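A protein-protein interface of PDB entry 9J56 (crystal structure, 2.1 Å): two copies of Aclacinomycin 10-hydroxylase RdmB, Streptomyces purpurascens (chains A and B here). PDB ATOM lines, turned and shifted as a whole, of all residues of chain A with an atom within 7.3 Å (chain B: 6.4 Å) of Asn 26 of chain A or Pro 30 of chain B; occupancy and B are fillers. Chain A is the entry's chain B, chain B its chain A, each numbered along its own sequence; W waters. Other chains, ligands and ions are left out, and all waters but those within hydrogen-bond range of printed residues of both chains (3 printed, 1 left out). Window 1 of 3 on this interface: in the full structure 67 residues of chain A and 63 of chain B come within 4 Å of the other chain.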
ATOM      1  N   VAL A  19     -27.103 -13.749 -28.568  1.00  0.00           N
ATOM      2  CA  VAL A  19     -26.480 -12.951 -27.522  1.00  0.00           C
ATOM      3  C   VAL A  19     -24.978 -13.222 -27.472  1.00  0.00           C
ATOM      4  O   VAL A  19     -24.162 -12.293 -27.385  1.00  0.00           O
ATOM      5  CB  VAL A  19     -27.168 -13.231 -26.173  1.00  0.00           C
ATOM      6  CG1 VAL A  19     -26.416 -12.549 -25.028  1.00  0.00           C
ATOM      7  CG2 VAL A  19     -28.617 -12.755 -26.216  1.00  0.00           C
ATOM      8  N   LEU A  20     -24.584 -14.495 -27.559  1.00  0.00           N
ATOM      9  CA  LEU A  20     -23.158 -14.812 -27.546  1.00  0.00           C
ATOM     10  C   LEU A  20     -22.442 -14.183 -28.738  1.00  0.00           C
ATOM     11  O   LEU A  20     -21.364 -13.588 -28.582  1.00  0.00           O
ATOM     12  CB  LEU A  20     -22.951 -16.329 -27.544  1.00  0.00           C
ATOM     13  CG  LEU A  20     -21.480 -16.762 -27.506  1.00  0.00           C
ATOM     14  CD1 LEU A  20     -20.771 -16.118 -26.315  1.00  0.00           C
ATOM     15  CD2 LEU A  20     -21.368 -18.293 -27.430  1.00  0.00           C
ATOM     16  N   LEU A  21     -23.044 -14.275 -29.932  1.00  0.00           N
ATOM     17  CA  LEU A  21     -22.343 -13.856 -31.146  1.00  0.00           C
ATOM     18  C   LEU A  21     -22.282 -12.337 -31.274  1.00  0.00           C
ATOM     19  O   LEU A  21     -21.261 -11.787 -31.703  1.00  0.00           O
ATOM     20  CB  LEU A  21     -23.016 -14.479 -32.381  1.00  0.00           C
ATOM     21  CG  LEU A  21     -22.856 -15.997 -32.529  1.00  0.00           C
ATOM     22  CD1 LEU A  21     -23.672 -16.575 -33.719  1.00  0.00           C
ATOM     23  CD2 LEU A  21     -21.390 -16.367 -32.652  1.00  0.00           C
ATOM     24  N   LYS A  22     -23.365 -11.641 -30.919  1.00  0.00           N
ATOM     25  CA  LYS A  22     -23.448 -10.198 -31.111  1.00  0.00           C
ATOM     26  C   LYS A  22     -23.005  -9.391 -29.902  1.00  0.00           C
ATOM     27  O   LYS A  22     -22.634  -8.225 -30.063  1.00  0.00           O
ATOM     28  CB  LYS A  22     -24.884  -9.779 -31.453  1.00  0.00           C
ATOM     29  CG  LYS A  22     -25.434 -10.448 -32.700  1.00  0.00           C
ATOM     30  CD  LYS A  22     -26.713  -9.765 -33.161  1.00  0.00           C
ATOM     31  CE  LYS A  22     -27.083 -10.246 -34.553  1.00  0.00           C
ATOM     32  NZ  LYS A  22     -28.552 -10.179 -34.753  1.00  0.00           N
ATOM     33  N   ASN A  23     -23.054  -9.968 -28.704  1.00  0.00           N
ATOM     34  CA  ASN A  23     -22.752  -9.238 -27.478  1.00  0.00           C
ATOM     35  C   ASN A  23     -21.570  -9.844 -26.715  1.00  0.00           C
ATOM     36  O   ASN A  23     -20.463  -9.296 -26.755  1.00  0.00           O
ATOM     37  CB  ASN A  23     -24.008  -9.201 -26.593  1.00  0.00           C
ATOM     38  CG  ASN A  23     -23.816  -8.400 -25.323  1.00  0.00           C
ATOM     39  OD1 ASN A  23     -22.693  -8.045 -24.960  1.00  0.00           O
ATOM     40  ND2 ASN A  23     -24.915  -8.120 -24.625  1.00  0.00           N
ATOM     41  N   LEU A  24     -21.795 -10.971 -26.015  1.00  0.00           N
ATOM     42  CA  LEU A  24     -20.871 -11.392 -24.953  1.00  0.00           C
ATOM     43  C   LEU A  24     -19.526 -11.850 -25.491  1.00  0.00           C
ATOM     44  O   LEU A  24     -18.504 -11.648 -24.832  1.00  0.00           O
ATOM     45  CB  LEU A  24     -21.474 -12.520 -24.111  1.00  0.00           C
ATOM     46  CG  LEU A  24     -22.769 -12.248 -23.342  1.00  0.00           C
ATOM     47  CD1 LEU A  24     -23.265 -13.545 -22.659  1.00  0.00           C
ATOM     48  CD2 LEU A  24     -22.580 -11.133 -22.341  1.00  0.00           C
ATOM     49  N   GLY A  25     -19.492 -12.475 -26.662  1.00  0.00           N
ATOM     50  CA  GLY A  25     -18.235 -12.870 -27.262  1.00  0.00           C
ATOM     51  C   GLY A  25     -17.773 -11.983 -28.397  1.00  0.00           C
ATOM     52  O   GLY A  25     -16.785 -12.312 -29.058  1.00  0.00           O
ATOM     53  N   ASN A  26     -18.455 -10.874 -28.646  1.00  0.00           N
ATOM     54  CA  ASN A  26     -18.161 -10.001 -29.777  1.00  0.00           C
ATOM     55  C   ASN A  26     -17.011  -9.049 -29.423  1.00  0.00           C
ATOM     56  O   ASN A  26     -17.188  -8.087 -28.668  1.00  0.00           O
ATOM     57  CB  ASN A  26     -19.432  -9.251 -30.164  1.00  0.00           C
ATOM     58  CG  ASN A  26     -19.232  -8.310 -31.335  1.00  0.00           C
ATOM     59  OD1 ASN A  26     -18.124  -8.177 -31.867  1.00  0.00           O
ATOM     60  ND2 ASN A  26     -20.314  -7.637 -31.740  1.00  0.00           N
ATOM     61  N   LEU A  27     -15.841  -9.294 -30.014  1.00  0.00           N
ATOM     62  CA  LEU A  27     -14.673  -8.440 -29.845  1.00  0.00           C
ATOM     63  C   LEU A  27     -14.546  -7.361 -30.923  1.00  0.00           C
ATOM     64  O   LEU A  27     -13.876  -6.337 -30.696  1.00  0.00           O
ATOM     65  CB  LEU A  27     -13.414  -9.309 -29.847  1.00  0.00           C
ATOM     66  CG  LEU A  27     -12.114  -8.734 -29.298  1.00  0.00           C
ATOM     67  CD1 LEU A  27     -12.223  -8.526 -27.792  1.00  0.00           C
ATOM     68  CD2 LEU A  27     -10.979  -9.684 -29.629  1.00  0.00           C
ATOM     69  N   VAL A  28     -15.179  -7.568 -32.077  1.00  0.00           N
ATOM     70  CA  VAL A  28     -15.042  -6.657 -33.211  1.00  0.00           C
ATOM     71  C   VAL A  28     -15.757  -5.340 -32.940  1.00  0.00           C
ATOM     72  O   VAL A  28     -15.227  -4.251 -33.208  1.00  0.00           O
ATOM     73  CB  VAL A  28     -15.583  -7.330 -34.484  1.00  0.00           C
ATOM     74  CG1 VAL A  28     -15.593  -6.343 -35.647  1.00  0.00           C
ATOM     75  CG2 VAL A  28     -14.744  -8.549 -34.802  1.00  0.00           C
ATOM     76  N   THR A  29     -16.976  -5.418 -32.428  1.00  0.00           N
ATOM     77  CA  THR A  29     -17.783  -4.216 -32.275  1.00  0.00           C
ATOM     78  C   THR A  29     -17.197  -3.249 -31.241  1.00  0.00           C
ATOM     79  O   THR A  29     -17.243  -2.035 -31.471  1.00  0.00           O
ATOM     80  CB  THR A  29     -19.224  -4.601 -31.933  1.00  0.00           C
ATOM     81  OG1 THR A  29     -19.809  -5.273 -33.062  1.00  0.00           O
ATOM     82  CG2 THR A  29     -20.058  -3.374 -31.576  1.00  0.00           C
ATOM     83  N   PRO A  30     -16.653  -3.711 -30.102  1.00  0.00           N
ATOM     84  CA  PRO A  30     -15.977  -2.746 -29.204  1.00  0.00           C
ATOM     85  C   PRO A  30     -14.763  -2.097 -29.827  1.00  0.00           C
ATOM     86  O   PRO A  30     -14.486  -0.925 -29.540  1.00  0.00           O
ATOM     87  CB  PRO A  30     -15.599  -3.577 -27.966  1.00  0.00           C
ATOM     88  CG  PRO A  30     -15.986  -4.991 -28.262  1.00  0.00           C
ATOM     89  CD  PRO A  30     -16.919  -4.991 -29.429  1.00  0.00           C
ATOM     90  N   MET A  31     -14.017  -2.810 -30.673  1.00  0.00           N
ATOM     91  CA  MET A  31     -12.920  -2.123 -31.343  1.00  0.00           C
ATOM     92  C   MET A  31     -13.431  -1.131 -32.380  1.00  0.00           C
ATOM     93  O   MET A  31     -12.847  -0.054 -32.549  1.00  0.00           O
ATOM     94  CB  MET A  31     -11.938  -3.118 -31.949  1.00  0.00           C
ATOM     95  CG  MET A  31     -11.157  -3.848 -30.863  1.00  0.00           C
ATOM     96  SD  MET A  31     -10.041  -2.786 -29.889  1.00  0.00           S
ATOM     97  CE  MET A  31      -9.476  -1.609 -31.120  1.00  0.00           C
ATOM     98  N   HIS A  72     -20.649  -1.617 -40.620  1.00  0.00           N
ATOM     99  CA  HIS A  72     -20.765  -2.276 -39.322  1.00  0.00           C
ATOM    100  C   HIS A  72     -21.381  -1.363 -38.270  1.00  0.00           C
ATOM    101  O   HIS A  72     -22.259  -1.781 -37.504  1.00  0.00           O
ATOM    102  CB  HIS A  72     -19.396  -2.751 -38.850  1.00  0.00           C
ATOM    103  CG  HIS A  72     -19.461  -3.634 -37.641  1.00  0.00           C
ATOM    104  ND1 HIS A  72     -20.049  -4.880 -37.666  1.00  0.00           N
ATOM    105  CD2 HIS A  72     -19.017  -3.451 -36.374  1.00  0.00           C
ATOM    106  CE1 HIS A  72     -19.968  -5.426 -36.464  1.00  0.00           C
ATOM    107  NE2 HIS A  72     -19.352  -4.577 -35.663  1.00  0.00           N
ATOM    108  N   VAL A  76     -24.954  -2.109 -36.049  1.00  0.00           N
ATOM    109  CA  VAL A  76     -25.027  -2.239 -34.592  1.00  0.00           C
ATOM    110  C   VAL A  76     -25.700  -1.051 -33.927  1.00  0.00           C
ATOM    111  O   VAL A  76     -25.779  -1.005 -32.693  1.00  0.00           O
ATOM    112  CB  VAL A  76     -23.629  -2.473 -33.980  1.00  0.00           C
ATOM    113  CG1 VAL A  76     -23.015  -3.760 -34.552  1.00  0.00           C
ATOM    114  CG2 VAL A  76     -22.711  -1.288 -34.224  1.00  0.00           C
ATOM    115  N   LEU A 126      -5.477 -11.554 -21.299  1.00  0.00           N
ATOM    116  CA  LEU A 126      -6.241 -12.003 -20.134  1.00  0.00           C
ATOM    117  C   LEU A 126      -5.924 -13.440 -19.745  1.00  0.00           C
ATOM    118  O   LEU A 126      -6.073 -13.806 -18.573  1.00  0.00           O
ATOM    119  CB  LEU A 126      -7.743 -11.882 -20.391  1.00  0.00           C
ATOM    120  CG  LEU A 126      -8.623 -12.153 -19.160  1.00  0.00           C
ATOM    121  CD1 LEU A 126      -8.188 -11.234 -17.987  1.00  0.00           C
ATOM    122  CD2 LEU A 126     -10.077 -11.938 -19.505  1.00  0.00           C
ATOM    123  N   ASN B  23     -22.362  -3.671 -23.637  1.00  0.00           N
ATOM    124  CA  ASN B  23     -22.409  -4.427 -24.885  1.00  0.00           C
ATOM    125  C   ASN B  23     -21.465  -3.832 -25.928  1.00  0.00           C
ATOM    126  O   ASN B  23     -20.359  -4.345 -26.125  1.00  0.00           O
ATOM    127  CB  ASN B  23     -23.862  -4.480 -25.390  1.00  0.00           C
ATOM    128  CG  ASN B  23     -24.033  -5.230 -26.732  1.00  0.00           C
ATOM    129  OD1 ASN B  23     -23.080  -5.501 -27.452  1.00  0.00           O
ATOM    130  ND2 ASN B  23     -25.276  -5.546 -27.059  1.00  0.00           N
ATOM    131  N   LEU B  24     -21.882  -2.743 -26.588  1.00  0.00           N
ATOM    132  CA  LEU B  24     -21.234  -2.327 -27.831  1.00  0.00           C
ATOM    133  C   LEU B  24     -19.785  -1.890 -27.623  1.00  0.00           C
ATOM    134  O   LEU B  24     -18.943  -2.089 -28.505  1.00  0.00           O
ATOM    135  CB  LEU B  24     -22.024  -1.194 -28.487  1.00  0.00           C
ATOM    136  CG  LEU B  24     -23.473  -1.431 -28.903  1.00  0.00           C
ATOM    137  CD1 LEU B  24     -24.047  -0.116 -29.403  1.00  0.00           C
ATOM    138  CD2 LEU B  24     -23.558  -2.492 -29.992  1.00  0.00           C
ATOM    139  N   ASN B  26     -17.905  -2.854 -24.913  1.00  0.00           N
ATOM    140  CA  ASN B  26     -17.387  -3.698 -23.842  1.00  0.00           C
ATOM    141  C   ASN B  26     -16.372  -4.664 -24.438  1.00  0.00           C
ATOM    142  O   ASN B  26     -16.740  -5.615 -25.138  1.00  0.00           O
ATOM    143  CB  ASN B  26     -18.556  -4.420 -23.165  1.00  0.00           C
ATOM    144  CG  ASN B  26     -18.126  -5.437 -22.118  1.00  0.00           C
ATOM    145  OD1 ASN B  26     -16.944  -5.639 -21.873  1.00  0.00           O
ATOM    146  ND2 ASN B  26     -19.107  -6.094 -21.501  1.00  0.00           N
ATOM    147  N   LEU B  27     -15.099  -4.415 -24.157  1.00  0.00           N
ATOM    148  CA  LEU B  27     -13.983  -5.243 -24.590  1.00  0.00           C
ATOM    149  C   LEU B  27     -13.614  -6.304 -23.575  1.00  0.00           C
ATOM    150  O   LEU B  27     -12.911  -7.258 -23.921  1.00  0.00           O
ATOM    151  CB  LEU B  27     -12.744  -4.369 -24.830  1.00  0.00           C
ATOM    152  CG  LEU B  27     -11.627  -4.835 -25.754  1.00  0.00           C
ATOM    153  CD1 LEU B  27     -12.172  -5.032 -27.173  1.00  0.00           C
ATOM    154  CD2 LEU B  27     -10.476  -3.819 -25.752  1.00  0.00           C
ATOM    155  N   VAL B  28     -14.059  -6.147 -22.330  1.00  0.00           N
ATOM    156  CA  VAL B  28     -13.635  -7.046 -21.268  1.00  0.00           C
ATOM    157  C   VAL B  28     -14.383  -8.372 -21.352  1.00  0.00           C
ATOM    158  O   VAL B  28     -13.775  -9.446 -21.360  1.00  0.00           O
ATOM    159  CB  VAL B  28     -13.831  -6.365 -19.899  1.00  0.00           C
ATOM    160  CG1 VAL B  28     -13.443  -7.305 -18.763  1.00  0.00           C
ATOM    161  CG2 VAL B  28     -12.996  -5.077 -19.822  1.00  0.00           C
ATOM    162  N   THR B  29     -15.712  -8.319 -21.413  1.00  0.00           N
ATOM    163  CA  THR B  29     -16.491  -9.555 -21.412  1.00  0.00           C
ATOM    164  C   THR B  29     -16.120 -10.485 -22.565  1.00  0.00           C
ATOM    165  O   THR B  29     -15.901 -11.681 -22.306  1.00  0.00           O
ATOM    166  CB  THR B  29     -17.984  -9.214 -21.394  1.00  0.00           C
ATOM    167  OG1 THR B  29     -18.280  -8.415 -20.239  1.00  0.00           O
ATOM    168  CG2 THR B  29     -18.836 -10.492 -21.362  1.00  0.00           C
ATOM    169  N   PRO B  30     -15.978 -10.033 -23.817  1.00  0.00           N
ATOM    170  CA  PRO B  30     -15.526 -10.975 -24.864  1.00  0.00           C
ATOM    171  C   PRO B  30     -14.177 -11.615 -24.596  1.00  0.00           C
ATOM    172  O   PRO B  30     -13.963 -12.757 -25.005  1.00  0.00           O
ATOM    173  CB  PRO B  30     -15.494 -10.112 -26.135  1.00  0.00           C
ATOM    174  CG  PRO B  30     -15.538  -8.692 -25.655  1.00  0.00           C
ATOM    175  CD  PRO B  30     -16.334  -8.724 -24.399  1.00  0.00           C
ATOM    176  N   MET B  31     -13.247 -10.937 -23.918  1.00  0.00           N
ATOM    177  CA  MET B  31     -12.004 -11.617 -23.597  1.00  0.00           C
ATOM    178  C   MET B  31     -12.214 -12.646 -22.494  1.00  0.00           C
ATOM    179  O   MET B  31     -11.575 -13.707 -22.503  1.00  0.00           O
ATOM    180  CB  MET B  31     -10.919 -10.608 -23.206  1.00  0.00           C
ATOM    181  CG  MET B  31     -10.402  -9.832 -24.402  1.00  0.00           C
ATOM    182  SD  MET B  31      -9.743 -10.882 -25.739  1.00  0.00           S
ATOM    183  CE  MET B  31      -8.870 -12.190 -24.872  1.00  0.00           C
ATOM    184  N   ALA B  32     -13.104 -12.352 -21.543  1.00  0.00           N
ATOM    185  CA  ALA B  32     -13.428 -13.329 -20.508  1.00  0.00           C
ATOM    186  C   ALA B  32     -14.078 -14.572 -21.117  1.00  0.00           C
ATOM    187  O   ALA B  32     -13.808 -15.707 -20.697  1.00  0.00           O
ATOM    188  CB  ALA B  32     -14.359 -12.690 -19.473  1.00  0.00           C
ATOM    189  N   LEU B  33     -14.925 -14.378 -22.125  1.00  0.00           N
ATOM    190  CA  LEU B  33     -15.520 -15.526 -22.801  1.00  0.00           C
ATOM    191  C   LEU B  33     -14.447 -16.371 -23.472  1.00  0.00           C
ATOM    192  O   LEU B  33     -14.491 -17.604 -23.415  1.00  0.00           O
ATOM    193  CB  LEU B  33     -16.554 -15.060 -23.823  1.00  0.00           C
ATOM    194  CG  LEU B  33     -18.006 -15.032 -23.344  1.00  0.00           C
ATOM    195  CD1 LEU B  33     -18.513 -16.436 -23.084  1.00  0.00           C
ATOM    196  CD2 LEU B  33     -18.122 -14.176 -22.086  1.00  0.00           C
ATOM    197  N   ARG B  34     -13.479 -15.722 -24.113  1.00  0.00           N
ATOM    198  CA  ARG B  34     -12.412 -16.447 -24.784  1.00  0.00           C
ATOM    199  C   ARG B  34     -11.523 -17.169 -23.783  1.00  0.00           C
ATOM    200  O   ARG B  34     -11.118 -18.313 -24.024  1.00  0.00           O
ATOM    201  CB  ARG B  34     -11.590 -15.493 -25.646  1.00  0.00           C
ATOM    202  CG  ARG B  34     -12.304 -15.133 -26.941  1.00  0.00           C
ATOM    203  CD  ARG B  34     -11.647 -13.954 -27.656  1.00  0.00           C
ATOM    204  NE  ARG B  34     -12.233 -13.749 -28.979  1.00  0.00           N
ATOM    205  CZ  ARG B  34     -13.409 -13.177 -29.197  1.00  0.00           C
ATOM    206  NH1 ARG B  34     -14.158 -12.737 -28.201  1.00  0.00           N
ATOM    207  NH2 ARG B  34     -13.855 -13.060 -30.443  1.00  0.00           N
ATOM    208  N   VAL B  35     -11.199 -16.529 -22.653  1.00  0.00           N
ATOM    209  CA  VAL B  35     -10.450 -17.255 -21.627  1.00  0.00           C
ATOM    210  C   VAL B  35     -11.275 -18.434 -21.095  1.00  0.00           C
ATOM    211  O   VAL B  35     -10.738 -19.526 -20.865  1.00  0.00           O
ATOM    212  CB  VAL B  35     -10.003 -16.303 -20.501  1.00  0.00           C
ATOM    213  CG1 VAL B  35      -9.457 -17.097 -19.319  1.00  0.00           C
ATOM    214  CG2 VAL B  35      -8.947 -15.299 -21.029  1.00  0.00           C
ATOM    215  N   HIS B  72     -17.260 -12.504 -12.861  1.00  0.00           N
ATOM    216  CA  HIS B  72     -17.688 -11.745 -14.033  1.00  0.00           C
ATOM    217  C   HIS B  72     -18.584 -12.588 -14.930  1.00  0.00           C
ATOM    218  O   HIS B  72     -19.606 -12.100 -15.435  1.00  0.00           O
ATOM    219  CB  HIS B  72     -16.492 -11.238 -14.829  1.00  0.00           C
ATOM    220  CG  HIS B  72     -16.881 -10.360 -15.979  1.00  0.00           C
ATOM    221  ND1 HIS B  72     -17.345  -9.074 -15.807  1.00  0.00           N
ATOM    222  CD2 HIS B  72     -16.904 -10.591 -17.314  1.00  0.00           C
ATOM    223  CE1 HIS B  72     -17.626  -8.545 -16.984  1.00  0.00           C
ATOM    224  NE2 HIS B  72     -17.367  -9.444 -17.917  1.00  0.00           N
ATOM    225  N   LEU B 110     -13.938 -19.655 -30.013  1.00  0.00           N
ATOM    226  CA  LEU B 110     -13.451 -18.697 -29.032  1.00  0.00           C
ATOM    227  C   LEU B 110     -12.118 -19.097 -28.395  1.00  0.00           C
ATOM    228  O   LEU B 110     -11.484 -18.254 -27.751  1.00  0.00           O
ATOM    229  CB  LEU B 110     -14.499 -18.525 -27.937  1.00  0.00           C
ATOM    230  CG  LEU B 110     -15.816 -17.875 -28.336  1.00  0.00           C
ATOM    231  CD1 LEU B 110     -16.846 -18.158 -27.253  1.00  0.00           C
ATOM    232  CD2 LEU B 110     -15.588 -16.369 -28.511  1.00  0.00           C
ATOM    233  N   PHE B 299     -25.630  -7.998 -39.675  1.00  0.00           N
ATOM    234  CA  PHE B 299     -24.600  -8.082 -38.644  1.00  0.00           C
ATOM    235  C   PHE B 299     -23.508  -9.055 -39.055  1.00  0.00           C
ATOM    236  O   PHE B 299     -22.314  -8.754 -38.945  1.00  0.00           O
ATOM    237  CB  PHE B 299     -25.172  -8.504 -37.292  1.00  0.00           C
ATOM    238  CG  PHE B 299     -24.107  -8.669 -36.236  1.00  0.00           C
ATOM    239  CD1 PHE B 299     -23.629  -7.562 -35.551  1.00  0.00           C
ATOM    240  CD2 PHE B 299     -23.546  -9.907 -35.977  1.00  0.00           C
ATOM    241  CE1 PHE B 299     -22.634  -7.693 -34.601  1.00  0.00           C
ATOM    242  CE2 PHE B 299     -22.554 -10.050 -35.030  1.00  0.00           C
ATOM    243  CZ  PHE B 299     -22.095  -8.922 -34.337  1.00  0.00           C
ATOM    244  N   LEU B 303     -19.553  -8.276 -39.820  1.00  0.00           N
ATOM    245  CA  LEU B 303     -18.596  -8.892 -38.908  1.00  0.00           C
ATOM    246  C   LEU B 303     -17.576  -9.721 -39.675  1.00  0.00           C
ATOM    247  O   LEU B 303     -16.369  -9.579 -39.471  1.00  0.00           O
ATOM    248  CB  LEU B 303     -19.333  -9.758 -37.884  1.00  0.00           C
ATOM    249  CG  LEU B 303     -18.471 -10.619 -36.963  1.00  0.00           C
ATOM    250  CD1 LEU B 303     -17.821  -9.756 -35.924  1.00  0.00           C
ATOM    251  CD2 LEU B 303     -19.292 -11.706 -36.273  1.00  0.00           C
HETATM  252  O   HOH W   1     -20.272  -7.642 -23.990  1.00  0.00           O
HETATM  253  O   HOH W   2     -15.888 -11.401 -32.200  1.00  0.00           O
HETATM  254  O   HOH W   3     -20.722  -6.078 -28.798  1.00  0.00           O
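Hydrophobic or aromatic side chains of chain A within 4 Å of the printed part of chain B: Leu 20, Leu 24, Leu 27, Val 28, Pro 30, His 72, Val 76 and Leu 126. Of the 16 printed residues of chain B, 13 touch a printed residue of chain A. Hydrophobic or aromatic side chains of chain B within 4 Å of the printed part of chain A: Leu 24, Leu 27, Pro 30, Met 31, Leu 33, Val 35, Phe 299 and Leu 303. Along chain B the printed residues that touch a printed residue of chain A span positions 23 to 303. Among the printed residues, 27 pairs touch across the chains. Among the printed residues, no Asp or Glu carboxylate lies within 4 Å of a Lys or Arg side-chain nitrogen of the other chain.
The backbone carbonyl oxygen (O) of Leu 24 of chain B lies close to the backbone carbonyl oxygen (O) of Thr 29 of chain A, 3.4 Å away. The guanidinium group (NH1) of Arg 34 of chain B sits at hydrogen-bond distance from the backbone carbonyl oxygen (O) of Gly 25 of chain A (2.8 Å). The backbone carbonyl oxygen (O) of Leu 24 of chain A sits close to the backbone nitrogen (N) of Pro 30 of chain B (3.2 Å). The backbone nitrogen (N) of Pro 30 of chain A sits close to the backbone carbonyl oxygen (O) of Leu 24 of chain B (3.2 Å).
Of the printed residues of chain B, Leu 21 of chain A touches Phe 299 (3.97 Å). Printed residues of chain B within 4 Å of Asn 26 of chain A: Pro 30 (3.5 Å) and Phe 299 (3.4 Å). Of the printed residues of chain B, Val 76 of chain A touches Leu 24 and Phe 299. Of the printed residues of chain A, Leu 27 of chain B touches Leu 27 (3.5 Å) and Pro 30 (3.8 Å). Of the printed residues of chain A, Thr 29 of chain B touches Leu 24 (3.5 Å). Of chain A, only Leu 24, Gly 25, Asn 26 and Leu 27 come within 4 Å of Pro 30 of chain B. Of the printed residues of chain A, Leu 303 of chain B touches Val 28 (3.5 Å).
Asn 23 of chain B touches its own counterpart, Asn 23 of chain A. Leu 24 of chain A touches Pro 30 of chain B, and with the chains exchanged Pro 30 of chain A touches Leu 24 of chain B. Asn 26 of chain A touches Pro 30 of chain B, and with the chains exchanged Pro 30 of chain A touches Asn 26 of chain B. Leu 27 of chain A touches Pro 30 of chain B, and with the chains exchanged Pro 30 of chain A touches Leu 27 of chain B. 9 positions are printed for both chains.
Leu 21 of chain A touches Phe 299 of chain B (O to CE2, 3.97 Å). Lys 22 of chain A touches Phe 299 of chain B (CA to CZ, 3.7 Å). O of Asn 26 of chain A touches CG of Pro 30 of chain B, at 3.5 Å. Asn 26 of chain A touches Phe 299 of chain B (ND2 to CZ, 3.4 Å). CG of Pro 30 of chain B touches CD1 of Leu 27 of chain A, 3.9 Å away. SD of Met 31 of chain B touches CD1 of Leu 27 of chain A (3.99 Å). Pro 30 of chain A touches Leu 27 of chain B. Val 76 of chain A touches Leu 24 of chain B (O to CD2, 3.8 Å). CD2 of Leu 126 of chain A touches C of Met 31 of chain B, 3.7 Å away. Ala 32 of chain B touches Leu 126 of chain A.
Water W1 bridges the side-chain amide oxygen (OD1) of Asn 23 of chain A (2.6 Å) and the side-chain amide nitrogen (ND2) of Asn 26 of chain B (3.2 Å). Water W3 lies within hydrogen-bond range of OD1 of Asn 23 of chain B (2.8 Å), O of Lys 22 of chain A (3.1 Å) and ND2 of Asn 26 of chain A (3.4 Å). Water W2 lies within hydrogen-bond range of N of Leu 27 of chain A, NH2 of Arg 34 of chain B and O of Gly 25 of chain A.
The backbone carbonyl oxygen (O) of Val 19 of chain A sits at hydrogen-bond distance from the backbone NH (N) of Leu 24 of chain A, 3.0 Å away. The side-chain hydroxyl of Thr 29 of chain B sits at hydrogen-bond distance from a ring nitrogen (NE2) of His 72 of chain B (2.7 Å). OG1 of Thr 29 of chain A is in hydrogen-bond range of ND2 of Asn 26 of chain A (2.8 Å). OG1 of Thr 29 of chain A lies within hydrogen-bond range of NE2 of His 72 of chain A. The side-chain amide nitrogen (ND2) of Asn 26 of chain A lies within hydrogen-bond range of the backbone carbonyl oxygen (O) of Lys 22 of chain A (2.9 Å). The side-chain amide nitrogen (ND2) of Asn 26 of chain B is in hydrogen-bond range of the side-chain hydroxyl (OG1) of Thr 29 of chain B (2.8 Å).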
